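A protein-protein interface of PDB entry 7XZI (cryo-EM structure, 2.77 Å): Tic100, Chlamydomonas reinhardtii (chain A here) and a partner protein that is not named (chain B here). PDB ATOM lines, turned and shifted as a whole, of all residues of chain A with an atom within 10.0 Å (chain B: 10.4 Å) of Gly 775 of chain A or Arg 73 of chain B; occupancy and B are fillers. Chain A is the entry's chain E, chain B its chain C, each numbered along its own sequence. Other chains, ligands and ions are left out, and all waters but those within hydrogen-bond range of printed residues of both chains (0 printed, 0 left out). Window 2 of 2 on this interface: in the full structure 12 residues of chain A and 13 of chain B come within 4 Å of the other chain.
Hydrophobic or aromatic side chains of chain A that line the printed part of chain B: His 771, Pro 773 and His 774.
Printed residues of chain B that touch a printed residue of chain A: Ser 65, Cys 66, Glu 69, Met 72 and Arg 73.
Hydrophobic or aromatic side chains of chain B that line the printed part of chain A: Met 72.
Among the printed residues, 8 pairs touch across the chains.
A ring nitrogen (ND1) of His 771 of chain A is in hydrogen-bond range of the side-chain hydroxyl of Ser 65 of chain B (2.6 Å).
A ring nitrogen (NE2) of His 771 of chain A lies within hydrogen-bond range of the side-chain sulfur (SG) of Cys 66 of chain B, at 3.4 Å.
A ring nitrogen (NE2) of His 771 of chain A lies within hydrogen-bond range of the side-chain carboxylate of Glu 69 of chain B (2.9 Å).
The side-chain carboxylate of Glu 69 of chain B lies within hydrogen-bond range of the backbone NH of His 774 of chain A (3.0 Å).
The backbone NH (N) of His 774 of chain A sits close to the guanidinium group (NH2) of Arg 73 of chain B (3.4 Å).
Among the printed residues, merely in contact across the chains: Pro 773 of chain A with Glu 69 of chain B, His 774 of chain A with Met 72 of chain B and Gly 775 of chain A with Arg 73 of chain B.
Printed residues of chain B within 4 Å of His 771 of chain A: Ser 65, Cys 66 and Glu 69.
Of chain B, only Glu 69, Met 72 and Arg 73 come within 4 Å of His 774 of chain A.
Of the printed residues of chain A, Cys 66 of chain B touches His 771.
No residue of chain A comes within 4 Å of Gln 70 of chain B.
Of chain A, only His 774 comes within 4 Å of Met 72 of chain B.
Arg 73 of chain B touches just these residues of chain A: His 774 (3.4 Å) and Gly 775 (3.6 Å).
No residue of chain A comes within 4 Å of Ala 76 of chain B.
The nearest residue of chain A that does not touch Arg 73 of chain B is Pro 773 of chain A (4.5 Å).
The nearest printed residue of chain A that does not touch Ser 65 of chain B is Pro 773 of chain A (4.8 Å).
The side-chain hydroxyl of Thr 776 of chain A is in hydrogen-bond range of the backbone carbonyl oxygen of Pro 773 of chain A.
OE2 of Glu 69 of chain B is in salt-bridge range of NH2 of Arg 73 of chain B (2.7 Å).
The side-chain amide oxygen (OE1) of Gln 70 of chain B sits at hydrogen-bond distance from the guanidinium group (NH1) of Arg 73 of chain B (3.4 Å).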
ATOM      1  N   MET A 766      18.269  -7.859  23.979  1.00  0.00           N
ATOM      2  CA  MET A 766      16.956  -8.502  23.963  1.00  0.00           C
ATOM      3  C   MET A 766      17.023  -9.767  24.813  1.00  0.00           C
ATOM      4  O   MET A 766      17.187 -10.886  24.323  1.00  0.00           O
ATOM      5  CB  MET A 766      16.519  -8.809  22.536  1.00  0.00           C
ATOM      6  CG  MET A 766      16.324  -7.576  21.675  1.00  0.00           C
ATOM      7  SD  MET A 766      15.738  -7.968  20.015  1.00  0.00           S
ATOM      8  CE  MET A 766      15.596  -6.324  19.320  1.00  0.00           C
ATOM      9  N   HIS A 771       9.210  -9.853  26.863  1.00  0.00           N
ATOM     10  CA  HIS A 771       9.090  -8.943  25.731  1.00  0.00           C
ATOM     11  C   HIS A 771       9.981  -9.421  24.592  1.00  0.00           C
ATOM     12  O   HIS A 771      11.178  -9.654  24.791  1.00  0.00           O
ATOM     13  CB  HIS A 771       9.455  -7.518  26.142  1.00  0.00           C
ATOM     14  CG  HIS A 771       9.062  -6.478  25.138  1.00  0.00           C
ATOM     15  ND1 HIS A 771       9.942  -5.527  24.669  1.00  0.00           N
ATOM     16  CD2 HIS A 771       7.883  -6.238  24.517  1.00  0.00           C
ATOM     17  CE1 HIS A 771       9.323  -4.745  23.803  1.00  0.00           C
ATOM     18  NE2 HIS A 771       8.074  -5.157  23.691  1.00  0.00           N
ATOM     19  N   TYR A 772       9.392  -9.564  23.403  1.00  0.00           N
ATOM     20  CA  TYR A 772      10.103  -9.931  22.179  1.00  0.00           C
ATOM     21  C   TYR A 772       9.821  -8.854  21.141  1.00  0.00           C
ATOM     22  O   TYR A 772       8.840  -8.946  20.387  1.00  0.00           O
ATOM     23  CB  TYR A 772       9.669 -11.309  21.682  1.00  0.00           C
ATOM     24  CG  TYR A 772      10.077 -12.445  22.592  1.00  0.00           C
ATOM     25  CD1 TYR A 772       9.361 -12.730  23.746  1.00  0.00           C
ATOM     26  CD2 TYR A 772      11.179 -13.234  22.296  1.00  0.00           C
ATOM     27  CE1 TYR A 772       9.732 -13.763  24.579  1.00  0.00           C
ATOM     28  CE2 TYR A 772      11.557 -14.272  23.124  1.00  0.00           C
ATOM     29  CZ  TYR A 772      10.829 -14.532  24.264  1.00  0.00           C
ATOM     30  OH  TYR A 772      11.200 -15.565  25.094  1.00  0.00           O
ATOM     31  N   PRO A 773      10.652  -7.815  21.064  1.00  0.00           N
ATOM     32  CA  PRO A 773      10.316  -6.665  20.216  1.00  0.00           C
ATOM     33  C   PRO A 773      10.809  -6.776  18.783  1.00  0.00           C
ATOM     34  O   PRO A 773      11.566  -7.688  18.437  1.00  0.00           O
ATOM     35  CB  PRO A 773      11.001  -5.504  20.941  1.00  0.00           C
ATOM     36  CG  PRO A 773      12.213  -6.132  21.535  1.00  0.00           C
ATOM     37  CD  PRO A 773      11.842  -7.556  21.892  1.00  0.00           C
ATOM     38  N   HIS A 774      10.377  -5.825  17.950  1.00  0.00           N
ATOM     39  CA  HIS A 774      10.859  -5.672  16.575  1.00  0.00           C
ATOM     40  C   HIS A 774      10.680  -6.951  15.761  1.00  0.00           C
ATOM     41  O   HIS A 774      11.556  -7.355  14.997  1.00  0.00           O
ATOM     42  CB  HIS A 774      12.317  -5.212  16.561  1.00  0.00           C
ATOM     43  CG  HIS A 774      12.538  -3.904  17.253  1.00  0.00           C
ATOM     44  ND1 HIS A 774      12.212  -2.694  16.679  1.00  0.00           N
ATOM     45  CD2 HIS A 774      13.043  -3.617  18.476  1.00  0.00           C
ATOM     46  CE1 HIS A 774      12.509  -1.718  17.518  1.00  0.00           C
ATOM     47  NE2 HIS A 774      13.015  -2.251  18.615  1.00  0.00           N
ATOM     48  N   GLY A 775       9.525  -7.588  15.929  1.00  0.00           N
ATOM     49  CA  GLY A 775       9.199  -8.773  15.149  1.00  0.00           C
ATOM     50  C   GLY A 775      10.154  -9.930  15.346  1.00  0.00           C
ATOM     51  O   GLY A 775      10.522 -10.602  14.374  1.00  0.00           O
ATOM     52  N   THR A 776      10.566 -10.180  16.587  1.00  0.00           N
ATOM     53  CA  THR A 776      11.426 -11.309  16.919  1.00  0.00           C
ATOM     54  C   THR A 776      10.695 -12.334  17.778  1.00  0.00           C
ATOM     55  O   THR A 776      11.323 -13.091  18.522  1.00  0.00           O
ATOM     56  CB  THR A 776      12.695 -10.836  17.627  1.00  0.00           C
ATOM     57  OG1 THR A 776      12.343 -10.168  18.844  1.00  0.00           O
ATOM     58  CG2 THR A 776      13.485  -9.887  16.741  1.00  0.00           C
ATOM     59  N   LYS A 777       9.364 -12.367  17.687  1.00  0.00           N
ATOM     60  CA  LYS A 777       8.577 -13.290  18.494  1.00  0.00           C
ATOM     61  C   LYS A 777       8.747 -14.740  18.064  1.00  0.00           C
ATOM     62  O   LYS A 777       8.304 -15.636  18.790  1.00  0.00           O
ATOM     63  CB  LYS A 777       7.098 -12.908  18.444  1.00  0.00           C
ATOM     64  CG  LYS A 777       6.826 -11.455  18.796  1.00  0.00           C
ATOM     65  CD  LYS A 777       5.338 -11.181  18.926  1.00  0.00           C
ATOM     66  CE  LYS A 777       5.073  -9.695  19.108  1.00  0.00           C
ATOM     67  NZ  LYS A 777       5.839  -9.134  20.254  1.00  0.00           N
ATOM     68  N   PHE A 778       9.367 -14.992  16.909  1.00  0.00           N
ATOM     69  CA  PHE A 778       9.662 -16.359  16.501  1.00  0.00           C
ATOM     70  C   PHE A 778      10.727 -17.009  17.372  1.00  0.00           C
ATOM     71  O   PHE A 778      10.896 -18.230  17.307  1.00  0.00           O
ATOM     72  CB  PHE A 778      10.102 -16.389  15.035  1.00  0.00           C
ATOM     73  CG  PHE A 778      11.437 -15.745  14.784  1.00  0.00           C
ATOM     74  CD1 PHE A 778      11.539 -14.375  14.613  1.00  0.00           C
ATOM     75  CD2 PHE A 778      12.588 -16.512  14.709  1.00  0.00           C
ATOM     76  CE1 PHE A 778      12.766 -13.782  14.379  1.00  0.00           C
ATOM     77  CE2 PHE A 778      13.815 -15.925  14.476  1.00  0.00           C
ATOM     78  CZ  PHE A 778      13.904 -14.558  14.311  1.00  0.00           C
ATOM     79  N   MET A 779      11.444 -16.226  18.180  1.00  0.00           N
ATOM     80  CA  MET A 779      12.453 -16.769  19.079  1.00  0.00           C
ATOM     81  C   MET A 779      11.862 -17.325  20.366  1.00  0.00           C
ATOM     82  O   MET A 779      12.603 -17.906  21.164  1.00  0.00           O
ATOM     83  CB  MET A 779      13.486 -15.693  19.424  1.00  0.00           C
ATOM     84  CG  MET A 779      14.194 -15.097  18.222  1.00  0.00           C
ATOM     85  SD  MET A 779      15.396 -13.840  18.693  1.00  0.00           S
ATOM     86  CE  MET A 779      16.057 -13.393  17.090  1.00  0.00           C
ATOM     87  N   ALA A 780      10.567 -17.161  20.588  1.00  0.00           N
ATOM     88  CA  ALA A 780       9.943 -17.655  21.809  1.00  0.00           C
ATOM     89  C   ALA A 780       9.964 -19.176  21.824  1.00  0.00           C
ATOM     90  O   ALA A 780       9.460 -19.804  20.885  1.00  0.00           O
ATOM     91  CB  ALA A 780       8.513 -17.139  21.917  1.00  0.00           C
ATOM     92  N   LEU A 784       3.887 -19.697  21.216  1.00  0.00           N
ATOM     93  CA  LEU A 784       3.818 -18.355  20.646  1.00  0.00           C
ATOM     94  C   LEU A 784       4.770 -18.205  19.467  1.00  0.00           C
ATOM     95  O   LEU A 784       4.489 -17.456  18.525  1.00  0.00           O
ATOM     96  CB  LEU A 784       4.129 -17.313  21.722  1.00  0.00           C
ATOM     97  CG  LEU A 784       3.953 -15.843  21.334  1.00  0.00           C
ATOM     98  CD1 LEU A 784       2.477 -15.483  21.245  1.00  0.00           C
ATOM     99  CD2 LEU A 784       4.683 -14.925  22.306  1.00  0.00           C
ATOM    100  N   GLY A 785       5.904 -18.904  19.505  1.00  0.00           N
ATOM    101  CA  GLY A 785       6.866 -18.797  18.421  1.00  0.00           C
ATOM    102  C   GLY A 785       6.344 -19.352  17.108  1.00  0.00           C
ATOM    103  O   GLY A 785       6.636 -18.816  16.037  1.00  0.00           O
ATOM    104  N   HIS A 788       4.312 -16.996  14.630  1.00  0.00           N
ATOM    105  CA  HIS A 788       5.015 -16.040  13.789  1.00  0.00           C
ATOM    106  C   HIS A 788       6.002 -16.758  12.872  1.00  0.00           C
ATOM    107  O   HIS A 788       6.302 -17.941  13.040  1.00  0.00           O
ATOM    108  CB  HIS A 788       5.731 -15.000  14.653  1.00  0.00           C
ATOM    109  CG  HIS A 788       4.815 -14.263  15.580  1.00  0.00           C
ATOM    110  ND1 HIS A 788       4.279 -13.031  15.273  1.00  0.00           N
ATOM    111  CD2 HIS A 788       4.326 -14.592  16.799  1.00  0.00           C
ATOM    112  CE1 HIS A 788       3.507 -12.630  16.266  1.00  0.00           C
ATOM    113  NE2 HIS A 788       3.518 -13.559  17.204  1.00  0.00           N
ATOM    114  N   ALA A 789       6.508 -16.016  11.892  1.00  0.00           N
ATOM    115  CA  ALA A 789       7.353 -16.564  10.843  1.00  0.00           C
ATOM    116  C   ALA A 789       8.794 -16.099  11.005  1.00  0.00           C
ATOM    117  O   ALA A 789       9.076 -15.058  11.602  1.00  0.00           O
ATOM    118  CB  ALA A 789       6.831 -16.164   9.459  1.00  0.00           C
ATOM    119  N   VAL A 790       9.707 -16.893  10.455  1.00  0.00           N
ATOM    120  CA  VAL A 790      11.139 -16.609  10.505  1.00  0.00           C
ATOM    121  C   VAL A 790      11.486 -15.583   9.430  1.00  0.00           C
ATOM    122  O   VAL A 790      10.774 -15.481   8.421  1.00  0.00           O
ATOM    123  CB  VAL A 790      11.957 -17.900  10.343  1.00  0.00           C
ATOM    124  CG1 VAL A 790      11.752 -18.802  11.549  1.00  0.00           C
ATOM    125  CG2 VAL A 790      11.554 -18.618   9.068  1.00  0.00           C
ATOM    126  N   PRO A 791      12.559 -14.807   9.595  1.00  0.00           N
ATOM    127  CA  PRO A 791      12.864 -13.727   8.648  1.00  0.00           C
ATOM    128  C   PRO A 791      13.424 -14.181   7.308  1.00  0.00           C
ATOM    129  O   PRO A 791      13.873 -13.330   6.535  1.00  0.00           O
ATOM    130  CB  PRO A 791      13.911 -12.891   9.409  1.00  0.00           C
ATOM    131  CG  PRO A 791      13.797 -13.310  10.842  1.00  0.00           C
ATOM    132  CD  PRO A 791      13.422 -14.749  10.785  1.00  0.00           C
ATOM    133  N   ASP A 792      13.417 -15.484   7.011  1.00  0.00           N
ATOM    134  CA  ASP A 792      13.846 -16.010   5.710  1.00  0.00           C
ATOM    135  C   ASP A 792      15.311 -15.685   5.423  1.00  0.00           C
ATOM    136  O   ASP A 792      15.636 -14.992   4.455  1.00  0.00           O
ATOM    137  CB  ASP A 792      12.943 -15.501   4.579  1.00  0.00           C
ATOM    138  CG  ASP A 792      13.167 -16.241   3.268  1.00  0.00           C
ATOM    139  OD1 ASP A 792      13.893 -17.257   3.266  1.00  0.00           O
ATOM    140  OD2 ASP A 792      12.615 -15.804   2.237  1.00  0.00           O
ATOM    141  N   LEU A 796      20.533 -17.928   9.293  1.00  0.00           N
ATOM    142  CA  LEU A 796      19.720 -17.959  10.503  1.00  0.00           C
ATOM    143  C   LEU A 796      18.984 -19.287  10.630  1.00  0.00           C
ATOM    144  O   LEU A 796      18.872 -19.843  11.729  1.00  0.00           O
ATOM    145  CB  LEU A 796      18.735 -16.790  10.497  1.00  0.00           C
ATOM    146  CG  LEU A 796      18.038 -16.446  11.815  1.00  0.00           C
ATOM    147  CD1 LEU A 796      19.053 -15.993  12.851  1.00  0.00           C
ATOM    148  CD2 LEU A 796      16.976 -15.380  11.602  1.00  0.00           C
ATOM    149  N   SER B  65      10.532  -0.914  27.818  1.00  0.00           N
ATOM    150  CA  SER B  65      10.925  -1.598  26.592  1.00  0.00           C
ATOM    151  C   SER B  65       9.866  -1.445  25.509  1.00  0.00           C
ATOM    152  O   SER B  65      10.196  -1.182  24.347  1.00  0.00           O
ATOM    153  CB  SER B  65      11.193  -3.073  26.881  1.00  0.00           C
ATOM    154  OG  SER B  65      11.602  -3.754  25.709  1.00  0.00           O
ATOM    155  N   CYS B  66       8.588  -1.599  25.867  1.00  0.00           N
ATOM    156  CA  CYS B  66       7.526  -1.440  24.877  1.00  0.00           C
ATOM    157  C   CYS B  66       7.492  -0.015  24.336  1.00  0.00           C
ATOM    158  O   CYS B  66       7.355   0.202  23.123  1.00  0.00           O
ATOM    159  CB  CYS B  66       6.177  -1.819  25.486  1.00  0.00           C
ATOM    160  SG  CYS B  66       6.028  -3.560  25.953  1.00  0.00           S
ATOM    161  N   CYS B  67       7.614   0.974  25.224  1.00  0.00           N
ATOM    162  CA  CYS B  67       7.583   2.365  24.787  1.00  0.00           C
ATOM    163  C   CYS B  67       8.775   2.689  23.895  1.00  0.00           C
ATOM    164  O   CYS B  67       8.628   3.382  22.882  1.00  0.00           O
ATOM    165  CB  CYS B  67       7.545   3.294  26.001  1.00  0.00           C
ATOM    166  SG  CYS B  67       6.878   4.939  25.662  1.00  0.00           S
ATOM    167  N   ASN B  68       9.964   2.194  24.250  1.00  0.00           N
ATOM    168  CA  ASN B  68      11.142   2.416  23.419  1.00  0.00           C
ATOM    169  C   ASN B  68      10.984   1.756  22.058  1.00  0.00           C
ATOM    170  O   ASN B  68      11.357   2.332  21.031  1.00  0.00           O
ATOM    171  CB  ASN B  68      12.396   1.896  24.122  1.00  0.00           C
ATOM    172  CG  ASN B  68      12.945   2.873  25.141  1.00  0.00           C
ATOM    173  OD1 ASN B  68      13.571   3.871  24.787  1.00  0.00           O
ATOM    174  ND2 ASN B  68      12.725   2.581  26.416  1.00  0.00           N
ATOM    175  N   GLU B  69      10.439   0.537  22.030  1.00  0.00           N
ATOM    176  CA  GLU B  69      10.208  -0.143  20.761  1.00  0.00           C
ATOM    177  C   GLU B  69       9.277   0.667  19.869  1.00  0.00           C
ATOM    178  O   GLU B  69       9.566   0.891  18.687  1.00  0.00           O
ATOM    179  CB  GLU B  69       9.630  -1.534  21.012  1.00  0.00           C
ATOM    180  CG  GLU B  69       9.210  -2.267  19.751  1.00  0.00           C
ATOM    181  CD  GLU B  69       8.362  -3.487  20.044  1.00  0.00           C
ATOM    182  OE1 GLU B  69       7.939  -3.653  21.206  1.00  0.00           O
ATOM    183  OE2 GLU B  69       8.121  -4.281  19.112  1.00  0.00           O
ATOM    184  N   GLN B  70       8.154   1.125  20.428  1.00  0.00           N
ATOM    185  CA  GLN B  70       7.200   1.889  19.629  1.00  0.00           C
ATOM    186  C   GLN B  70       7.800   3.208  19.157  1.00  0.00           C
ATOM    187  O   GLN B  70       7.630   3.595  17.993  1.00  0.00           O
ATOM    188  CB  GLN B  70       5.921   2.126  20.430  1.00  0.00           C
ATOM    189  CG  GLN B  70       5.169   0.849  20.765  1.00  0.00           C
ATOM    190  CD  GLN B  70       4.672   0.130  19.527  1.00  0.00           C
ATOM    191  OE1 GLN B  70       4.681  -1.098  19.464  1.00  0.00           O
ATOM    192  NE2 GLN B  70       4.228   0.895  18.537  1.00  0.00           N
ATOM    193  N   GLY B  71       8.517   3.907  20.039  1.00  0.00           N
ATOM    194  CA  GLY B  71       9.120   5.170  19.651  1.00  0.00           C
ATOM    195  C   GLY B  71      10.176   5.008  18.577  1.00  0.00           C
ATOM    196  O   GLY B  71      10.241   5.799  17.633  1.00  0.00           O
ATOM    197  N   MET B  72      11.023   3.983  18.704  1.00  0.00           N
ATOM    198  CA  MET B  72      12.044   3.739  17.694  1.00  0.00           C
ATOM    199  C   MET B  72      11.421   3.339  16.363  1.00  0.00           C
ATOM    200  O   MET B  72      11.896   3.763  15.305  1.00  0.00           O
ATOM    201  CB  MET B  72      13.023   2.672  18.180  1.00  0.00           C
ATOM    202  CG  MET B  72      13.957   3.158  19.276  1.00  0.00           C
ATOM    203  SD  MET B  72      15.242   1.966  19.691  1.00  0.00           S
ATOM    204  CE  MET B  72      14.253   0.592  20.273  1.00  0.00           C
ATOM    205  N   ARG B  73      10.360   2.527  16.388  1.00  0.00           N
ATOM    206  CA  ARG B  73       9.659   2.203  15.150  1.00  0.00           C
ATOM    207  C   ARG B  73       9.118   3.461  14.485  1.00  0.00           C
ATOM    208  O   ARG B  73       9.295   3.665  13.278  1.00  0.00           O
ATOM    209  CB  ARG B  73       8.518   1.221  15.422  1.00  0.00           C
ATOM    210  CG  ARG B  73       8.922  -0.239  15.469  1.00  0.00           C
ATOM    211  CD  ARG B  73       7.779  -1.112  14.975  1.00  0.00           C
ATOM    212  NE  ARG B  73       7.993  -2.523  15.256  1.00  0.00           N
ATOM    213  CZ  ARG B  73       7.440  -3.174  16.274  1.00  0.00           C
ATOM    214  NH1 ARG B  73       6.633  -2.565  17.128  1.00  0.00           N
ATOM    215  NH2 ARG B  73       7.704  -4.466  16.437  1.00  0.00           N
ATOM    216  N   ARG B  74       8.458   4.321  15.264  1.00  0.00           N
ATOM    217  CA  ARG B  74       7.877   5.534  14.698  1.00  0.00           C
ATOM    218  C   ARG B  74       8.951   6.459  14.139  1.00  0.00           C
ATOM    219  O   ARG B  74       8.769   7.061  13.075  1.00  0.00           O
ATOM    220  CB  ARG B  74       7.038   6.255  15.751  1.00  0.00           C
ATOM    221  CG  ARG B  74       6.441   7.567  15.275  1.00  0.00           C
ATOM    222  CD  ARG B  74       5.551   8.179  16.338  1.00  0.00           C
ATOM    223  NE  ARG B  74       6.198   8.191  17.642  1.00  0.00           N
ATOM    224  CZ  ARG B  74       7.028   9.141  18.059  1.00  0.00           C
ATOM    225  NH1 ARG B  74       7.336  10.175  17.295  1.00  0.00           N
ATOM    226  NH2 ARG B  74       7.562   9.048  19.273  1.00  0.00           N
ATOM    227  N   GLU B  75      10.077   6.592  14.845  1.00  0.00           N
ATOM    228  CA  GLU B  75      11.149   7.460  14.367  1.00  0.00           C
ATOM    229  C   GLU B  75      11.816   6.890  13.120  1.00  0.00           C
ATOM    230  O   GLU B  75      12.154   7.637  12.196  1.00  0.00           O
ATOM    231  CB  GLU B  75      12.175   7.688  15.477  1.00  0.00           C
ATOM    232  CG  GLU B  75      11.655   8.542  16.624  1.00  0.00           C
ATOM    233  CD  GLU B  75      12.655   8.679  17.755  1.00  0.00           C
ATOM    234  OE1 GLU B  75      13.787   8.175  17.615  1.00  0.00           O
ATOM    235  OE2 GLU B  75      12.307   9.290  18.787  1.00  0.00           O
ATOM    236  N   ALA B  76      12.022   5.570  13.075  1.00  0.00           N
ATOM    237  CA  ALA B  76      12.625   4.955  11.897  1.00  0.00           C
ATOM    238  C   ALA B  76      11.724   5.096  10.680  1.00  0.00           C
ATOM    239  O   ALA B  76      12.199   5.384   9.576  1.00  0.00           O
ATOM    240  CB  ALA B  76      12.931   3.484  12.173  1.00  0.00           C
ATOM    241  N   LEU B  77      10.415   4.891  10.859  1.00  0.00           N
ATOM    242  CA  LEU B  77       9.492   5.031   9.739  1.00  0.00           C
ATOM    243  C   LEU B  77       9.413   6.470   9.246  1.00  0.00           C
ATOM    244  O   LEU B  77       9.098   6.705   8.073  1.00  0.00           O
ATOM    245  CB  LEU B  77       8.103   4.530  10.134  1.00  0.00           C
ATOM    246  CG  LEU B  77       7.992   3.033  10.421  1.00  0.00           C
ATOM    247  CD1 LEU B  77       6.563   2.659  10.773  1.00  0.00           C
ATOM    248  CD2 LEU B  77       8.485   2.225   9.234  1.00  0.00           C
ATOM    249  N   SER B  78       9.691   7.442  10.115  1.00  0.00           N
ATOM    250  CA  SER B  78       9.619   8.845   9.731  1.00  0.00           C
ATOM    251  C   SER B  78      10.854   9.324   8.982  1.00  0.00           C
ATOM    252  O   SER B  78      10.846  10.449   8.469  1.00  0.00           O
ATOM    253  CB  SER B  78       9.402   9.718  10.969  1.00  0.00           C
ATOM    254  OG  SER B  78       9.319  11.087  10.617  1.00  0.00           O
ATOM    255  N   GLY B  79      11.906   8.514   8.908  1.00  0.00           N
ATOM    256  CA  GLY B  79      13.098   8.899   8.183  1.00  0.00           C
ATOM    257  C   GLY B  79      14.186   9.531   9.019  1.00  0.00           C
ATOM    258  O   GLY B  79      14.894  10.417   8.527  1.00  0.00           O
ATOM    259  N   LYS B  80      14.347   9.105  10.270  1.00  0.00           N
ATOM    260  CA  LYS B  80      15.373   9.652  11.146  1.00  0.00           C
ATOM    261  C   LYS B  80      15.980   8.527  11.972  1.00  0.00           C
ATOM    262  O   LYS B  80      15.369   7.474  12.172  1.00  0.00           O
ATOM    263  CB  LYS B  80      14.811  10.745  12.067  1.00  0.00           C
ATOM    264  CG  LYS B  80      13.777  10.248  13.062  1.00  0.00           C
ATOM    265  CD  LYS B  80      13.177  11.394  13.860  1.00  0.00           C
ATOM    266  CE  LYS B  80      12.449  12.375  12.956  1.00  0.00           C
ATOM    267  NZ  LYS B  80      11.853  13.504  13.724  1.00  0.00           N
ATOM    268  N   LYS B  81      17.195   8.764  12.448  1.00  0.00           N
ATOM    269  CA  LYS B  81      17.888   7.766  13.252  1.00  0.00           C
ATOM    270  C   LYS B  81      17.218   7.647  14.617  1.00  0.00           C
ATOM    271  O   LYS B  81      17.069   8.654  15.318  1.00  0.00           O
ATOM    272  CB  LYS B  81      19.358   8.142  13.413  1.00  0.00           C
ATOM    273  CG  LYS B  81      20.092   8.312  12.093  1.00  0.00           C
ATOM    274  CD  LYS B  81      21.523   8.766  12.310  1.00  0.00           C
ATOM    275  CE  LYS B  81      22.234   8.978  10.985  1.00  0.00           C
ATOM    276  NZ  LYS B  81      23.625   9.465  11.181  1.00  0.00           N
ATOM    277  N   PRO B  82      16.801   6.451  15.023  1.00  0.00           N
ATOM    278  CA  PRO B  82      16.106   6.306  16.306  1.00  0.00           C
ATOM    279  C   PRO B  82      17.031   6.545  17.489  1.00  0.00           C
ATOM    280  O   PRO B  82      18.249   6.371  17.413  1.00  0.00           O
ATOM    281  CB  PRO B  82      15.608   4.858  16.275  1.00  0.00           C
ATOM    282  CG  PRO B  82      16.566   4.161  15.375  1.00  0.00           C
ATOM    283  CD  PRO B  82      16.947   5.164  14.323  1.00  0.00           C
ATOM    284  N   ASN B  83      16.425   6.951  18.602  1.00  0.00           N
ATOM    285  CA  ASN B  83      17.133   7.180  19.852  1.00  0.00           C
ATOM    286  C   ASN B  83      16.552   6.293  20.944  1.00  0.00           C
ATOM    287  O   ASN B  83      15.370   5.939  20.915  1.00  0.00           O
ATOM    288  CB  ASN B  83      17.052   8.649  20.280  1.00  0.00           C
ATOM    289  CG  ASN B  83      17.717   9.580  19.289  1.00  0.00           C
ATOM    290  OD1 ASN B  83      17.094  10.030  18.329  1.00  0.00           O
ATOM    291  ND2 ASN B  83      18.990   9.876  19.519  1.00  0.00           N
ATOM    292  N   LEU B  84      17.393   5.940  21.912  1.00  0.00           N
ATOM    293  CA  LEU B  84      17.008   5.076  23.021  1.00  0.00           C
ATOM    294  C   LEU B  84      16.978   5.895  24.305  1.00  0.00           C
ATOM    295  O   LEU B  84      18.002   6.455  24.709  1.00  0.00           O
ATOM    296  CB  LEU B  84      17.975   3.900  23.159  1.00  0.00           C
ATOM    297  CG  LEU B  84      17.717   2.939  24.320  1.00  0.00           C
ATOM    298  CD1 LEU B  84      16.408   2.198  24.112  1.00  0.00           C
ATOM    299  CD2 LEU B  84      18.874   1.965  24.482  1.00  0.00           C
